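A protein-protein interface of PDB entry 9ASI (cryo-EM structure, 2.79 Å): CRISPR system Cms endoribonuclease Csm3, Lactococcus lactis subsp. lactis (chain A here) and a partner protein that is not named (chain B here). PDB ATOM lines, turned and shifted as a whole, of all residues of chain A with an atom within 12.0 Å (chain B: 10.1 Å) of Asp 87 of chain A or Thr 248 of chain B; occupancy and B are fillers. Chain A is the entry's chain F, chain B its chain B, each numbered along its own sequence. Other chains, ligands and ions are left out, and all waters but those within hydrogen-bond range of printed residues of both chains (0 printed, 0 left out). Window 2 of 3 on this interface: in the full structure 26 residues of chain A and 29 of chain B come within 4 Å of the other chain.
The side-chain hydroxyl of Thr 248 of chain B sits at hydrogen-bond distance from the side-chain carboxylate of Asp 87 of chain A, at 2.7 Å.
ND2 of Asn 249 of chain B lies within hydrogen-bond range of O of Ala 247 of chain B, 2.4 Å away.
O of Lys 86 of chain A touches O of Thr 248 of chain B, at 3.98 Å.
Asn 249 of chain B touches Lys 86 of chain A (CB to O, 3.8 Å).
Asp 244 of chain B touches Ile 89 of chain A.
Ile 89 of chain A touches Asn 249 of chain B (CD1 to C, 3.6 Å).
CD1 of Ile 89 of chain A touches N of Leu 250 of chain B, at 3.99 Å.
Arg 91 of chain A touches Asp 244 of chain B (CG to OD2, 3.2 Å).
No residue of chain B comes within 4 Å of Lys 88 of chain A.
Printed residues of chain B within 4 Å of Ile 89 of chain A: Asp 244, Asn 249 and Leu 250.
Val 241 of chain B touches none of the printed residues of chain A.
Tyr 246 of chain B touches none of the printed residues of chain A.
No residue of chain A comes within 4 Å of Ala 247 of chain B.
Of the printed residues of chain A, Thr 248 of chain B touches Lys 86 and Asp 87.
Of chain A, only Lys 86 (3.8 Å) and Ile 89 (3.6 Å) come within 4 Å of Asn 249 of chain B.
Of the printed residues of chain A, Leu 250 of chain B touches Ile 89.
The nearest residue of chain B that does not touch Asp 87 of chain A is Asn 249 of chain B (5.0 Å).
The nearest printed residue of chain A that does not touch Thr 248 of chain B is Ile 89 of chain A (5.0 Å).
The nearest printed residue of chain B that does not touch Ile 89 of chain A is Ser 243 of chain B (4.5 Å).
Printed residues of chain B that touch a printed residue of chain A: Asp 244, Thr 248, Asn 249 and Leu 250.
Of the 13 printed residues of chain A, 4 touch a printed residue of chain B.
Among the printed residues, 7 pairs touch across the chains.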
ATOM      1  N   ASP A  73      18.436   9.830  32.546  1.00  0.00           N
ATOM      2  CA  ASP A  73      19.499  10.439  33.337  1.00  0.00           C
ATOM      3  C   ASP A  73      19.479  11.958  33.217  1.00  0.00           C
ATOM      4  O   ASP A  73      18.716  12.518  32.433  1.00  0.00           O
ATOM      5  CB  ASP A  73      20.862   9.895  32.910  1.00  0.00           C
ATOM      6  CG  ASP A  73      21.286   8.688  33.721  1.00  0.00           C
ATOM      7  OD1 ASP A  73      21.009   8.661  34.939  1.00  0.00           O
ATOM      8  OD2 ASP A  73      21.896   7.765  33.140  1.00  0.00           O
ATOM      9  N   ASP A  75      20.927  15.906  32.518  1.00  0.00           N
ATOM     10  CA  ASP A  75      21.441  16.514  31.296  1.00  0.00           C
ATOM     11  C   ASP A  75      22.933  16.264  31.142  1.00  0.00           C
ATOM     12  O   ASP A  75      23.419  16.055  30.027  1.00  0.00           O
ATOM     13  CB  ASP A  75      21.148  18.014  31.292  1.00  0.00           C
ATOM     14  CG  ASP A  75      21.697  18.711  30.062  1.00  0.00           C
ATOM     15  OD1 ASP A  75      21.355  18.291  28.938  1.00  0.00           O
ATOM     16  OD2 ASP A  75      22.472  19.678  30.220  1.00  0.00           O
ATOM     17  N   LEU A  78      23.620  12.508  30.075  1.00  0.00           N
ATOM     18  CA  LEU A  78      23.122  12.267  28.723  1.00  0.00           C
ATOM     19  C   LEU A  78      23.951  13.006  27.681  1.00  0.00           C
ATOM     20  O   LEU A  78      24.220  12.468  26.602  1.00  0.00           O
ATOM     21  CB  LEU A  78      21.654  12.670  28.621  1.00  0.00           C
ATOM     22  CG  LEU A  78      20.673  11.790  29.394  1.00  0.00           C
ATOM     23  CD1 LEU A  78      19.241  12.152  29.043  1.00  0.00           C
ATOM     24  CD2 LEU A  78      20.941  10.318  29.135  1.00  0.00           C
ATOM     25  N   GLY A  82      25.733  10.212  25.860  1.00  0.00           N
ATOM     26  CA  GLY A  82      24.745   9.979  24.827  1.00  0.00           C
ATOM     27  C   GLY A  82      23.397   9.581  25.407  1.00  0.00           C
ATOM     28  O   GLY A  82      23.226   9.394  26.611  1.00  0.00           O
ATOM     29  N   SER A  83      22.428   9.451  24.504  1.00  0.00           N
ATOM     30  CA  SER A  83      21.081   9.042  24.872  1.00  0.00           C
ATOM     31  C   SER A  83      20.310   8.683  23.614  1.00  0.00           C
ATOM     32  O   SER A  83      20.505   9.300  22.565  1.00  0.00           O
ATOM     33  CB  SER A  83      20.345  10.150  25.633  1.00  0.00           C
ATOM     34  OG  SER A  83      19.193   9.641  26.280  1.00  0.00           O
ATOM     35  N   SER A  84      19.452   7.664  23.720  1.00  0.00           N
ATOM     36  CA  SER A  84      18.527   7.370  22.633  1.00  0.00           C
ATOM     37  C   SER A  84      17.170   6.874  23.122  1.00  0.00           C
ATOM     38  O   SER A  84      16.501   6.149  22.379  1.00  0.00           O
ATOM     39  CB  SER A  84      19.113   6.324  21.701  1.00  0.00           C
ATOM     40  OG  SER A  84      19.098   5.050  22.313  1.00  0.00           O
ATOM     41  N   GLU A  85      16.745   7.231  24.336  1.00  0.00           N
ATOM     42  CA  GLU A  85      15.750   6.422  25.032  1.00  0.00           C
ATOM     43  C   GLU A  85      14.417   6.338  24.299  1.00  0.00           C
ATOM     44  O   GLU A  85      14.087   5.283  23.750  1.00  0.00           O
ATOM     45  CB  GLU A  85      15.536   6.972  26.443  1.00  0.00           C
ATOM     46  CG  GLU A  85      14.638   6.112  27.313  1.00  0.00           C
ATOM     47  CD  GLU A  85      14.643   6.549  28.763  1.00  0.00           C
ATOM     48  OE1 GLU A  85      15.424   7.460  29.107  1.00  0.00           O
ATOM     49  OE2 GLU A  85      13.868   5.981  29.560  1.00  0.00           O
ATOM     50  N   LYS A  86      13.649   7.421  24.270  1.00  0.00           N
ATOM     51  CA  LYS A  86      12.452   7.420  23.432  1.00  0.00           C
ATOM     52  C   LYS A  86      12.283   8.693  22.620  1.00  0.00           C
ATOM     53  O   LYS A  86      11.883   8.623  21.456  1.00  0.00           O
ATOM     54  CB  LYS A  86      11.202   7.187  24.298  1.00  0.00           C
ATOM     55  CG  LYS A  86      10.959   5.730  24.673  1.00  0.00           C
ATOM     56  CD  LYS A  86      11.007   4.813  23.456  1.00  0.00           C
ATOM     57  CE  LYS A  86       9.822   5.036  22.531  1.00  0.00           C
ATOM     58  NZ  LYS A  86       9.430   3.780  21.833  1.00  0.00           N
ATOM     59  N   ASP A  87      12.563   9.853  23.209  1.00  0.00           N
ATOM     60  CA  ASP A  87      12.433  11.130  22.521  1.00  0.00           C
ATOM     61  C   ASP A  87      13.685  11.973  22.713  1.00  0.00           C
ATOM     62  O   ASP A  87      14.096  12.712  21.814  1.00  0.00           O
ATOM     63  CB  ASP A  87      11.202  11.884  23.023  1.00  0.00           C
ATOM     64  CG  ASP A  87      10.962  13.176  22.272  1.00  0.00           C
ATOM     65  OD1 ASP A  87      10.296  13.138  21.217  1.00  0.00           O
ATOM     66  OD2 ASP A  87      11.446  14.230  22.735  1.00  0.00           O
ATOM     67  N   LYS A  88      14.293  11.868  23.896  1.00  0.00           N
ATOM     68  CA  LYS A  88      15.461  12.670  24.256  1.00  0.00           C
ATOM     69  C   LYS A  88      16.725  12.006  23.708  1.00  0.00           C
ATOM     70  O   LYS A  88      17.529  11.405  24.423  1.00  0.00           O
ATOM     71  CB  LYS A  88      15.521  12.860  25.767  1.00  0.00           C
ATOM     72  CG  LYS A  88      15.386  11.573  26.568  1.00  0.00           C
ATOM     73  CD  LYS A  88      14.971  11.846  28.002  1.00  0.00           C
ATOM     74  CE  LYS A  88      14.486  10.577  28.684  1.00  0.00           C
ATOM     75  NZ  LYS A  88      13.418   9.893  27.903  1.00  0.00           N
ATOM     76  N   ILE A  89      16.895  12.127  22.396  1.00  0.00           N
ATOM     77  CA  ILE A  89      18.061  11.578  21.716  1.00  0.00           C
ATOM     78  C   ILE A  89      19.156  12.637  21.734  1.00  0.00           C
ATOM     79  O   ILE A  89      19.067  13.651  21.041  1.00  0.00           O
ATOM     80  CB  ILE A  89      17.731  11.139  20.286  1.00  0.00           C
ATOM     81  CG1 ILE A  89      16.706  10.007  20.299  1.00  0.00           C
ATOM     82  CG2 ILE A  89      18.990  10.692  19.572  1.00  0.00           C
ATOM     83  CD1 ILE A  89      16.372   9.483  18.932  1.00  0.00           C
ATOM     84  N   ARG A  90      20.180  12.403  22.549  1.00  0.00           N
ATOM     85  CA  ARG A  90      21.379  13.223  22.605  1.00  0.00           C
ATOM     86  C   ARG A  90      22.523  12.358  22.106  1.00  0.00           C
ATOM     87  O   ARG A  90      22.589  11.171  22.437  1.00  0.00           O
ATOM     88  CB  ARG A  90      21.636  13.708  24.034  1.00  0.00           C
ATOM     89  CG  ARG A  90      22.714  14.753  24.177  1.00  0.00           C
ATOM     90  CD  ARG A  90      22.298  16.047  23.513  1.00  0.00           C
ATOM     91  NE  ARG A  90      23.408  16.983  23.397  1.00  0.00           N
ATOM     92  CZ  ARG A  90      23.702  17.907  24.302  1.00  0.00           C
ATOM     93  NH1 ARG A  90      22.974  18.059  25.396  1.00  0.00           N
ATOM     94  NH2 ARG A  90      24.747  18.703  24.100  1.00  0.00           N
ATOM     95  N   ARG A  91      23.421  12.925  21.299  1.00  0.00           N
ATOM     96  CA  ARG A  91      24.281  12.045  20.509  1.00  0.00           C
ATOM     97  C   ARG A  91      25.436  11.477  21.330  1.00  0.00           C
ATOM     98  O   ARG A  91      25.451  10.282  21.644  1.00  0.00           O
ATOM     99  CB  ARG A  91      24.810  12.798  19.283  1.00  0.00           C
ATOM    100  CG  ARG A  91      25.206  14.237  19.539  1.00  0.00           C
ATOM    101  CD  ARG A  91      25.958  14.801  18.348  1.00  0.00           C
ATOM    102  NE  ARG A  91      27.040  13.917  17.936  1.00  0.00           N
ATOM    103  CZ  ARG A  91      28.239  13.892  18.500  1.00  0.00           C
ATOM    104  NH1 ARG A  91      28.557  14.718  19.483  1.00  0.00           N
ATOM    105  NH2 ARG A  91      29.143  13.019  18.065  1.00  0.00           N
ATOM    106  N   VAL B 241      18.305   6.198  10.636  1.00  0.00           N
ATOM    107  CA  VAL B 241      18.955   7.489  10.470  1.00  0.00           C
ATOM    108  C   VAL B 241      19.707   7.827  11.751  1.00  0.00           C
ATOM    109  O   VAL B 241      19.119   7.891  12.835  1.00  0.00           O
ATOM    110  CB  VAL B 241      17.927   8.572  10.132  1.00  0.00           C
ATOM    111  CG1 VAL B 241      18.568   9.935  10.213  1.00  0.00           C
ATOM    112  CG2 VAL B 241      17.346   8.326   8.758  1.00  0.00           C
ATOM    113  N   SER B 243      20.982  10.475  13.605  1.00  0.00           N
ATOM    114  CA  SER B 243      21.042  11.886  13.952  1.00  0.00           C
ATOM    115  C   SER B 243      20.095  12.138  15.112  1.00  0.00           C
ATOM    116  O   SER B 243      19.028  11.528  15.192  1.00  0.00           O
ATOM    117  CB  SER B 243      20.686  12.788  12.766  1.00  0.00           C
ATOM    118  OG  SER B 243      19.576  12.285  12.053  1.00  0.00           O
ATOM    119  N   ASP B 244      20.498  13.036  16.002  1.00  0.00           N
ATOM    120  CA  ASP B 244      19.659  13.456  17.113  1.00  0.00           C
ATOM    121  C   ASP B 244      18.708  14.578  16.733  1.00  0.00           C
ATOM    122  O   ASP B 244      17.875  14.970  17.557  1.00  0.00           O
ATOM    123  CB  ASP B 244      20.533  13.898  18.287  1.00  0.00           C
ATOM    124  CG  ASP B 244      21.670  14.795  17.857  1.00  0.00           C
ATOM    125  OD1 ASP B 244      21.868  14.962  16.636  1.00  0.00           O
ATOM    126  OD2 ASP B 244      22.361  15.340  18.741  1.00  0.00           O
ATOM    127  N   THR B 245      18.816  15.100  15.512  1.00  0.00           N
ATOM    128  CA  THR B 245      17.962  16.185  15.051  1.00  0.00           C
ATOM    129  C   THR B 245      17.132  15.725  13.860  1.00  0.00           C
ATOM    130  O   THR B 245      17.045  16.428  12.852  1.00  0.00           O
ATOM    131  CB  THR B 245      18.795  17.409  14.665  1.00  0.00           C
ATOM    132  OG1 THR B 245      19.402  17.191  13.388  1.00  0.00           O
ATOM    133  CG2 THR B 245      19.886  17.653  15.687  1.00  0.00           C
ATOM    134  N   TYR B 246      16.539  14.537  13.961  1.00  0.00           N
ATOM    135  CA  TYR B 246      15.707  13.983  12.901  1.00  0.00           C
ATOM    136  C   TYR B 246      14.532  13.259  13.535  1.00  0.00           C
ATOM    137  O   TYR B 246      14.730  12.305  14.293  1.00  0.00           O
ATOM    138  CB  TYR B 246      16.512  13.025  12.018  1.00  0.00           C
ATOM    139  CG  TYR B 246      15.770  12.456  10.826  1.00  0.00           C
ATOM    140  CD1 TYR B 246      15.793  13.102   9.602  1.00  0.00           C
ATOM    141  CD2 TYR B 246      15.077  11.262  10.917  1.00  0.00           C
ATOM    142  CE1 TYR B 246      15.138  12.589   8.509  1.00  0.00           C
ATOM    143  CE2 TYR B 246      14.414  10.742   9.828  1.00  0.00           C
ATOM    144  CZ  TYR B 246      14.447  11.411   8.628  1.00  0.00           C
ATOM    145  OH  TYR B 246      13.785  10.889   7.542  1.00  0.00           O
ATOM    146  N   ALA B 247      13.320  13.731  13.250  1.00  0.00           N
ATOM    147  CA  ALA B 247      12.081  13.007  13.524  1.00  0.00           C
ATOM    148  C   ALA B 247      11.864  12.693  15.004  1.00  0.00           C
ATOM    149  O   ALA B 247      11.056  11.818  15.328  1.00  0.00           O
ATOM    150  CB  ALA B 247      12.010  11.712  12.707  1.00  0.00           C
ATOM    151  N   THR B 248      12.598  13.354  15.904  1.00  0.00           N
ATOM    152  CA  THR B 248      12.356  13.358  17.359  1.00  0.00           C
ATOM    153  C   THR B 248      12.189  11.954  17.954  1.00  0.00           C
ATOM    154  O   THR B 248      11.683  11.806  19.071  1.00  0.00           O
ATOM    155  CB  THR B 248      11.154  14.243  17.738  1.00  0.00           C
ATOM    156  OG1 THR B 248      11.198  14.524  19.141  1.00  0.00           O
ATOM    157  CG2 THR B 248       9.816  13.578  17.426  1.00  0.00           C
ATOM    158  N   ASN B 249      12.635  10.921  17.251  1.00  0.00           N
ATOM    159  CA  ASN B 249      12.595   9.548  17.745  1.00  0.00           C
ATOM    160  C   ASN B 249      13.500   8.714  16.848  1.00  0.00           C
ATOM    161  O   ASN B 249      14.174   9.239  15.957  1.00  0.00           O
ATOM    162  CB  ASN B 249      11.171   8.992  17.788  1.00  0.00           C
ATOM    163  CG  ASN B 249      10.490   9.022  16.436  1.00  0.00           C
ATOM    164  OD1 ASN B 249      10.698   8.139  15.605  1.00  0.00           O
ATOM    165  ND2 ASN B 249       9.660  10.036  16.214  1.00  0.00           N
ATOM    166  N   LEU B 250      13.511   7.408  17.087  1.00  0.00           N
ATOM    167  CA  LEU B 250      14.405   6.493  16.381  1.00  0.00           C
ATOM    168  C   LEU B 250      13.616   5.873  15.231  1.00  0.00           C
ATOM    169  O   LEU B 250      12.869   4.913  15.422  1.00  0.00           O
ATOM    170  CB  LEU B 250      14.955   5.437  17.333  1.00  0.00           C
ATOM    171  CG  LEU B 250      16.226   4.708  16.902  1.00  0.00           C
ATOM    172  CD1 LEU B 250      17.402   5.662  16.950  1.00  0.00           C
ATOM    173  CD2 LEU B 250      16.489   3.493  17.768  1.00  0.00           C
ATOM    174  N   VAL B 251      13.797   6.424  14.034  1.00  0.00           N
ATOM    175  CA  VAL B 251      13.020   6.060  12.856  1.00  0.00           C
ATOM    176  C   VAL B 251      13.955   5.494  11.796  1.00  0.00           C
ATOM    177  O   VAL B 251      15.091   5.953  11.648  1.00  0.00           O
ATOM    178  CB  VAL B 251      12.229   7.272  12.316  1.00  0.00           C
ATOM    179  CG1 VAL B 251      13.170   8.374  11.911  1.00  0.00           C
ATOM    180  CG2 VAL B 251      11.359   6.873  11.139  1.00  0.00           C
ATOM    181  N   LYS B 279      10.550  12.570   5.456  1.00  0.00           N
ATOM    182  CA  LYS B 279       9.575  12.993   6.451  1.00  0.00           C
ATOM    183  C   LYS B 279      10.225  13.685   7.640  1.00  0.00           C
ATOM    184  O   LYS B 279       9.524  14.347   8.412  1.00  0.00           O
ATOM    185  CB  LYS B 279       8.751  11.790   6.909  1.00  0.00           C
ATOM    186  CG  LYS B 279       8.048  11.071   5.766  1.00  0.00           C
ATOM    187  CD  LYS B 279       7.780   9.615   6.097  1.00  0.00           C
ATOM    188  CE  LYS B 279       7.721   8.771   4.834  1.00  0.00           C
ATOM    189  NZ  LYS B 279       7.148   7.420   5.087  1.00  0.00           N
ATOM    190  N   GLY B 280      11.538  13.549   7.805  1.00  0.00           N
ATOM    191  CA  GLY B 280      12.252  14.276   8.831  1.00  0.00           C
ATOM    192  C   GLY B 280      12.595  15.685   8.392  1.00  0.00           C
ATOM    193  O   GLY B 280      12.269  16.127   7.292  1.00  0.00           O
ATOM    194  N   ASN B 281      13.277  16.405   9.280  1.00  0.00           N
ATOM    195  CA  ASN B 281      13.530  17.823   9.072  1.00  0.00           C
ATOM    196  C   ASN B 281      14.937  18.119   8.568  1.00  0.00           C
ATOM    197  O   ASN B 281      15.346  19.284   8.567  1.00  0.00           O
ATOM    198  CB  ASN B 281      13.250  18.606  10.356  1.00  0.00           C
ATOM    199  CG  ASN B 281      13.866  17.969  11.571  1.00  0.00           C
ATOM    200  OD1 ASN B 281      15.070  17.745  11.618  1.00  0.00           O
ATOM    201  ND2 ASN B 281      13.041  17.673  12.569  1.00  0.00           N
ATOM    202  N   HIS B 282      15.687  17.107   8.147  1.00  0.00           N
ATOM    203  CA  HIS B 282      16.902  17.339   7.382  1.00  0.00           C
ATOM    204  C   HIS B 282      17.041  16.251   6.329  1.00  0.00           C
ATOM    205  O   HIS B 282      16.564  15.126   6.527  1.00  0.00           O
ATOM    206  CB  HIS B 282      18.160  17.389   8.267  1.00  0.00           C
ATOM    207  CG  HIS B 282      18.439  16.132   9.032  1.00  0.00           C
ATOM    208  ND1 HIS B 282      18.665  14.917   8.423  1.00  0.00           N
ATOM    209  CD2 HIS B 282      18.578  15.916  10.361  1.00  0.00           C
ATOM    210  CE1 HIS B 282      18.907  14.003   9.344  1.00  0.00           C
ATOM    211  NE2 HIS B 282      18.861  14.583  10.528  1.00  0.00           N
